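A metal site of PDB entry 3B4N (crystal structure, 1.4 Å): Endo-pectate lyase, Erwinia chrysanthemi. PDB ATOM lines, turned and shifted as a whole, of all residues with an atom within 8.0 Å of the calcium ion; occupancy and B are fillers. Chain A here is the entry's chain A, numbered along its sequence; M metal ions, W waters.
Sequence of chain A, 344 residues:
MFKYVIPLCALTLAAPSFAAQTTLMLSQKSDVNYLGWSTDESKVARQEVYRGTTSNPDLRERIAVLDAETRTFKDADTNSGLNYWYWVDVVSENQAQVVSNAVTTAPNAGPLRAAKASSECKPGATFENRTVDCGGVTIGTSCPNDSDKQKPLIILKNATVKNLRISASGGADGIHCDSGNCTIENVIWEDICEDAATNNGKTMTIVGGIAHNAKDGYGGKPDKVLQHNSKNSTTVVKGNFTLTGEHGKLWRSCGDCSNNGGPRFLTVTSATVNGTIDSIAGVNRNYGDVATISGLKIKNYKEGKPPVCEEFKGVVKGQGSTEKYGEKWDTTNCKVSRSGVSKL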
ATOM      1  N   CYS A 143       4.420  18.555 -34.655  1.00  0.00           N
ATOM      2  CA  CYS A 143       3.762  19.841 -34.695  1.00  0.00           C
ATOM      3  C   CYS A 143       4.315  20.588 -35.900  1.00  0.00           C
ATOM      4  O   CYS A 143       5.093  21.537 -35.765  1.00  0.00           O
ATOM      5  CB  CYS A 143       4.007  20.630 -33.411  1.00  0.00           C
ATOM      6  SG  CYS A 143       3.015  22.161 -33.316  1.00  0.00           S
ATOM      7  N   ALA A 168       7.409  18.992 -26.124  1.00  0.00           N
ATOM      8  CA  ALA A 168       7.488  20.307 -26.752  1.00  0.00           C
ATOM      9  C   ALA A 168       7.338  20.272 -28.261  1.00  0.00           C
ATOM     10  O   ALA A 168       6.745  21.172 -28.847  1.00  0.00           O
ATOM     11  CB  ALA A 168       8.797  20.994 -26.369  1.00  0.00           C
ATOM     12  N   GLU A 190       4.590  20.906 -22.677  1.00  0.00           N
ATOM     13  CA  GLU A 190       5.903  21.558 -22.783  1.00  0.00           C
ATOM     14  C   GLU A 190       5.967  22.723 -23.789  1.00  0.00           C
ATOM     15  O   GLU A 190       6.780  23.630 -23.645  1.00  0.00           O
ATOM     16  CB  GLU A 190       6.982  20.515 -23.066  1.00  0.00           C
ATOM     17  CG  GLU A 190       7.266  19.568 -21.870  1.00  0.00           C
ATOM     18  CD  GLU A 190       7.902  20.272 -20.675  1.00  0.00           C
ATOM     19  OE1 GLU A 190       8.639  21.270 -20.866  1.00  0.00           O
ATOM     20  OE2 GLU A 190       7.691  19.830 -19.525  1.00  0.00           O
ATOM     21  N   ASP A 191       5.086  22.695 -24.788  1.00  0.00           N
ATOM     22  CA  ASP A 191       4.966  23.753 -25.792  1.00  0.00           C
ATOM     23  C   ASP A 191       3.697  23.435 -26.558  1.00  0.00           C
ATOM     24  O   ASP A 191       3.708  22.618 -27.479  1.00  0.00           O
ATOM     25  CB  ASP A 191       6.163  23.791 -26.751  1.00  0.00           C
ATOM     26  CG  ASP A 191       6.113  24.988 -27.708  1.00  0.00           C
ATOM     27  OD1 ASP A 191       5.035  25.584 -27.880  1.00  0.00           O
ATOM     28  OD2 ASP A 191       7.163  25.325 -28.299  1.00  0.00           O
ATOM     29  N   ILE A 192       2.593  24.060 -26.169  1.00  0.00           N
ATOM     30  CA  ILE A 192       1.319  23.823 -26.819  1.00  0.00           C
ATOM     31  C   ILE A 192       1.470  23.938 -28.331  1.00  0.00           C
ATOM     32  O   ILE A 192       2.107  24.876 -28.817  1.00  0.00           O
ATOM     33  CB  ILE A 192       0.286  24.869 -26.378  1.00  0.00           C
ATOM     34  CG1 ILE A 192      -0.033  24.697 -24.900  1.00  0.00           C
ATOM     35  CG2 ILE A 192      -0.970  24.755 -27.241  1.00  0.00           C
ATOM     36  CD1 ILE A 192      -0.857  25.841 -24.330  1.00  0.00           C
ATOM     37  N   CYS A 193       0.903  22.989 -29.063  1.00  0.00           N
ATOM     38  CA  CYS A 193       0.962  23.024 -30.512  1.00  0.00           C
ATOM     39  C   CYS A 193      -0.278  23.786 -31.009  1.00  0.00           C
ATOM     40  O   CYS A 193      -0.313  25.020 -30.903  1.00  0.00           O
ATOM     41  CB  CYS A 193       1.023  21.596 -31.070  1.00  0.00           C
ATOM     42  SG  CYS A 193       1.143  21.512 -32.887  1.00  0.00           S
ATOM     43  N   GLU A 194      -1.305  23.108 -31.515  1.00  0.00           N
ATOM     44  CA  GLU A 194      -2.493  23.824 -31.990  1.00  0.00           C
ATOM     45  C   GLU A 194      -3.213  24.484 -30.822  1.00  0.00           C
ATOM     46  O   GLU A 194      -3.613  25.644 -30.874  1.00  0.00           O
ATOM     47  CB  GLU A 194      -3.446  22.864 -32.710  1.00  0.00           C
ATOM     48  CG  GLU A 194      -2.934  22.351 -34.045  1.00  0.00           C
ATOM     49  CD  GLU A 194      -2.690  23.463 -35.061  1.00  0.00           C
ATOM     50  OE1 GLU A 194      -3.431  24.461 -35.062  1.00  0.00           O
ATOM     51  OE2 GLU A 194      -1.753  23.322 -35.870  1.00  0.00           O
ATOM     52  N   ASP A 195      -3.398  23.704 -29.769  1.00  0.00           N
ATOM     53  CA  ASP A 195      -4.032  24.148 -28.532  1.00  0.00           C
ATOM     54  C   ASP A 195      -3.796  23.031 -27.534  1.00  0.00           C
ATOM     55  O   ASP A 195      -3.300  21.978 -27.908  1.00  0.00           O
ATOM     56  CB  ASP A 195      -5.550  24.414 -28.738  1.00  0.00           C
ATOM     57  CG  ASP A 195      -6.210  23.386 -29.646  1.00  0.00           C
ATOM     58  OD1 ASP A 195      -6.519  23.729 -30.798  1.00  0.00           O
ATOM     59  OD2 ASP A 195      -6.427  22.250 -29.204  1.00  0.00           O
ATOM     60  N   HIS A 212       2.871  25.453 -21.159  1.00  0.00           N
ATOM     61  CA  HIS A 212       3.832  26.390 -21.676  1.00  0.00           C
ATOM     62  C   HIS A 212       3.591  26.696 -23.146  1.00  0.00           C
ATOM     63  O   HIS A 212       3.128  25.843 -23.899  1.00  0.00           O
ATOM     64  CB  HIS A 212       5.250  25.816 -21.527  1.00  0.00           C
ATOM     65  CG  HIS A 212       6.338  26.771 -21.919  1.00  0.00           C
ATOM     66  ND1 HIS A 212       6.640  27.890 -21.175  1.00  0.00           N
ATOM     67  CD2 HIS A 212       7.183  26.769 -22.973  1.00  0.00           C
ATOM     68  CE1 HIS A 212       7.634  28.539 -21.758  1.00  0.00           C
ATOM     69  NE2 HIS A 212       7.979  27.875 -22.845  1.00  0.00           N
ATOM     70  N   ASN A 213       3.843  27.930 -23.533  1.00  0.00           N
ATOM     71  CA  ASN A 213       3.782  28.276 -24.946  1.00  0.00           C
ATOM     72  C   ASN A 213       4.842  29.338 -25.130  1.00  0.00           C
ATOM     73  O   ASN A 213       5.276  29.961 -24.164  1.00  0.00           O
ATOM     74  CB  ASN A 213       2.408  28.764 -25.406  1.00  0.00           C
ATOM     75  CG  ASN A 213       2.124  28.368 -26.849  1.00  0.00           C
ATOM     76  OD1 ASN A 213       3.038  27.971 -27.572  1.00  0.00           O
ATOM     77  ND2 ASN A 213       0.870  28.486 -27.284  1.00  0.00           N
ATOM     78  N   ALA A 214       5.300  29.527 -26.350  1.00  0.00           N
ATOM     79  CA  ALA A 214       6.349  30.519 -26.567  1.00  0.00           C
ATOM     80  C   ALA A 214       6.237  31.180 -27.918  1.00  0.00           C
ATOM     81  O   ALA A 214       5.810  30.570 -28.896  1.00  0.00           O
ATOM     82  CB  ALA A 214       7.715  29.857 -26.425  1.00  0.00           C
ATOM     83  N   LYS A 215       6.652  32.439 -27.970  1.00  0.00           N
ATOM     84  CA  LYS A 215       6.651  33.155 -29.229  1.00  0.00           C
ATOM     85  C   LYS A 215       7.725  32.463 -30.051  1.00  0.00           C
ATOM     86  O   LYS A 215       8.799  32.146 -29.540  1.00  0.00           O
ATOM     87  CB  LYS A 215       6.999  34.630 -28.999  1.00  0.00           C
ATOM     88  CG  LYS A 215       7.217  35.426 -30.292  1.00  0.00           C
ATOM     89  CD  LYS A 215       7.276  36.924 -30.024  1.00  0.00           C
ATOM     90  CE  LYS A 215       5.882  37.532 -29.863  1.00  0.00           C
ATOM     91  NZ  LYS A 215       5.081  36.925 -28.752  1.00  0.00           N
ATOM     92  N   ASP A 216       7.407  32.200 -31.308  1.00  0.00           N
ATOM     93  CA  ASP A 216       8.325  31.531 -32.233  1.00  0.00           C
ATOM     94  C   ASP A 216       8.522  30.049 -31.885  1.00  0.00           C
ATOM     95  O   ASP A 216       9.441  29.413 -32.368  1.00  0.00           O
ATOM     96  CB  ASP A 216       9.673  32.276 -32.234  1.00  0.00           C
ATOM     97  CG  ASP A 216      10.568  31.856 -33.390  1.00  0.00           C
ATOM     98  OD1 ASP A 216      10.031  31.543 -34.469  1.00  0.00           O
ATOM     99  OD2 ASP A 216      11.804  31.879 -33.221  1.00  0.00           O
ATOM    100  N   GLY A 217       7.639  29.503 -31.044  1.00  0.00           N
ATOM    101  CA  GLY A 217       7.744  28.098 -30.678  1.00  0.00           C
ATOM    102  C   GLY A 217       7.015  27.181 -31.645  1.00  0.00           C
ATOM    103  O   GLY A 217       6.614  27.586 -32.739  1.00  0.00           O
ATOM    104  N   TYR A 218       6.837  25.913 -31.247  1.00  0.00           N
ATOM    105  CA  TYR A 218       6.149  24.954 -32.102  1.00  0.00           C
ATOM    106  C   TYR A 218       4.689  25.335 -32.278  1.00  0.00           C
ATOM    107  O   TYR A 218       4.025  25.681 -31.304  1.00  0.00           O
ATOM    108  CB  TYR A 218       6.214  23.544 -31.514  1.00  0.00           C
ATOM    109  CG  TYR A 218       7.568  22.906 -31.610  1.00  0.00           C
ATOM    110  CD1 TYR A 218       8.514  23.088 -30.597  1.00  0.00           C
ATOM    111  CD2 TYR A 218       7.919  22.124 -32.706  1.00  0.00           C
ATOM    112  CE1 TYR A 218       9.775  22.489 -30.680  1.00  0.00           C
ATOM    113  CE2 TYR A 218       9.169  21.524 -32.797  1.00  0.00           C
ATOM    114  CZ  TYR A 218      10.085  21.714 -31.781  1.00  0.00           C
ATOM    115  OH  TYR A 218      11.324  21.103 -31.854  1.00  0.00           O
ATOM    116  N   GLY A 219       4.199  25.271 -33.513  1.00  0.00           N
ATOM    117  CA  GLY A 219       2.820  25.619 -33.774  1.00  0.00           C
ATOM    118  C   GLY A 219       2.611  27.066 -34.186  1.00  0.00           C
ATOM    119  O   GLY A 219       1.486  27.466 -34.475  1.00  0.00           O
ATOM    120  N   GLY A 220       3.683  27.855 -34.193  1.00  0.00           N
ATOM    121  CA  GLY A 220       3.566  29.253 -34.592  1.00  0.00           C
ATOM    122  C   GLY A 220       3.228  30.194 -33.458  1.00  0.00           C
ATOM    123  O   GLY A 220       3.456  29.878 -32.282  1.00  0.00           O
ATOM    124  N   LYS A 221       2.689  31.360 -33.798  1.00  0.00           N
ATOM    125  CA  LYS A 221       2.333  32.346 -32.798  1.00  0.00           C
ATOM    126  C   LYS A 221       1.301  31.786 -31.812  1.00  0.00           C
ATOM    127  O   LYS A 221       0.269  31.246 -32.214  1.00  0.00           O
ATOM    128  CB  LYS A 221       1.764  33.595 -33.477  1.00  0.00           C
ATOM    129  CG  LYS A 221       1.259  34.649 -32.498  1.00  0.00           C
ATOM    130  CD  LYS A 221       1.112  36.001 -33.158  1.00  0.00           C
ATOM    131  CE  LYS A 221       0.144  35.985 -34.309  1.00  0.00           C
ATOM    132  NZ  LYS A 221      -0.008  37.368 -34.854  1.00  0.00           N
ATOM    133  N   PRO A 222       1.583  31.916 -30.503  1.00  0.00           N
ATOM    134  CA  PRO A 222       0.673  31.408 -29.478  1.00  0.00           C
ATOM    135  C   PRO A 222      -0.758  31.891 -29.679  1.00  0.00           C
ATOM    136  O   PRO A 222      -1.008  33.073 -29.903  1.00  0.00           O
ATOM    137  CB  PRO A 222       1.280  31.945 -28.182  1.00  0.00           C
ATOM    138  CG  PRO A 222       2.740  31.943 -28.484  1.00  0.00           C
ATOM    139  CD  PRO A 222       2.772  32.514 -29.889  1.00  0.00           C
ATOM    140  N   ASP A 223      -1.691  30.950 -29.602  1.00  0.00           N
ATOM    141  CA  ASP A 223      -3.105  31.258 -29.780  1.00  0.00           C
ATOM    142  C   ASP A 223      -3.825  30.752 -28.531  1.00  0.00           C
ATOM    143  O   ASP A 223      -3.335  30.957 -27.413  1.00  0.00           O
ATOM    144  CB  ASP A 223      -3.638  30.576 -31.042  1.00  0.00           C
ATOM    145  CG  ASP A 223      -4.960  31.147 -31.520  1.00  0.00           C
ATOM    146  OD1 ASP A 223      -5.583  31.965 -30.814  1.00  0.00           O
ATOM    147  OD2 ASP A 223      -5.392  30.754 -32.634  1.00  0.00           O
ATOM    148  N   GLU A 246       4.667  32.599 -23.239  1.00  0.00           N
ATOM    149  CA  GLU A 246       3.860  33.583 -23.945  1.00  0.00           C
ATOM    150  C   GLU A 246       2.642  32.869 -24.531  1.00  0.00           C
ATOM    151  O   GLU A 246       2.797  31.876 -25.249  1.00  0.00           O
ATOM    152  CB  GLU A 246       4.661  34.227 -25.089  1.00  0.00           C
ATOM    153  CG  GLU A 246       5.913  34.995 -24.664  1.00  0.00           C
ATOM    154  CD  GLU A 246       7.111  34.102 -24.420  1.00  0.00           C
ATOM    155  OE1 GLU A 246       7.451  33.303 -25.321  1.00  0.00           O
ATOM    156  OE2 GLU A 246       7.716  34.207 -23.336  1.00  0.00           O
ATOM    157  N   HIS A 247       1.451  33.386 -24.244  1.00  0.00           N
ATOM    158  CA  HIS A 247       0.199  32.798 -24.705  1.00  0.00           C
ATOM    159  C   HIS A 247      -0.717  33.761 -25.448  1.00  0.00           C
ATOM    160  O   HIS A 247      -0.596  34.981 -25.303  1.00  0.00           O
ATOM    161  CB  HIS A 247      -0.567  32.253 -23.507  1.00  0.00           C
ATOM    162  CG  HIS A 247       0.060  31.057 -22.885  1.00  0.00           C
ATOM    163  ND1 HIS A 247      -0.374  29.772 -23.141  1.00  0.00           N
ATOM    164  CD2 HIS A 247       1.107  30.931 -22.035  1.00  0.00           C
ATOM    165  CE1 HIS A 247       0.375  28.909 -22.476  1.00  0.00           C
ATOM    166  NE2 HIS A 247       1.281  29.594 -21.795  1.00  0.00           N
HETATM  167 CA    CA M   1       3.510  26.592 -29.367  1.00  0.00          CA
HETATM  168  O   HOH W   1       1.338  27.161 -30.290  1.00  0.00           O
HETATM  169  O   HOH W   2       4.439  28.575 -30.310  1.00  0.00           O
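Within 4 Å of the calcium ion: Asp 191, Ile 192, Asn 213 and Tyr 218.
Water W1 lies within hydrogen-bond range of O of Cys 193 (2.8 Å) and ND2 of Asn 213 (3.3 Å).
The backbone carbonyl oxygen of Asn 213 lies within hydrogen-bond range of the backbone NH of Glu 246, 2.9 Å away. O of His 212 sits at hydrogen-bond distance from N of Ile 192, at 2.9 Å. The side-chain sulfur (SG) of Cys 143 is disulfide-bonded to the side-chain sulfur (SG) of Cys 193 (2.0 Å).
The calcium ion is bound by O of Tyr 218 (2.2 Å), O of Ile 192 (2.3 Å), OD1 of Asn 213 (2.3 Å), OD1 of Asp 191 (2.4 Å), water W2 (2.4 Å) and water W1 (2.4 Å).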
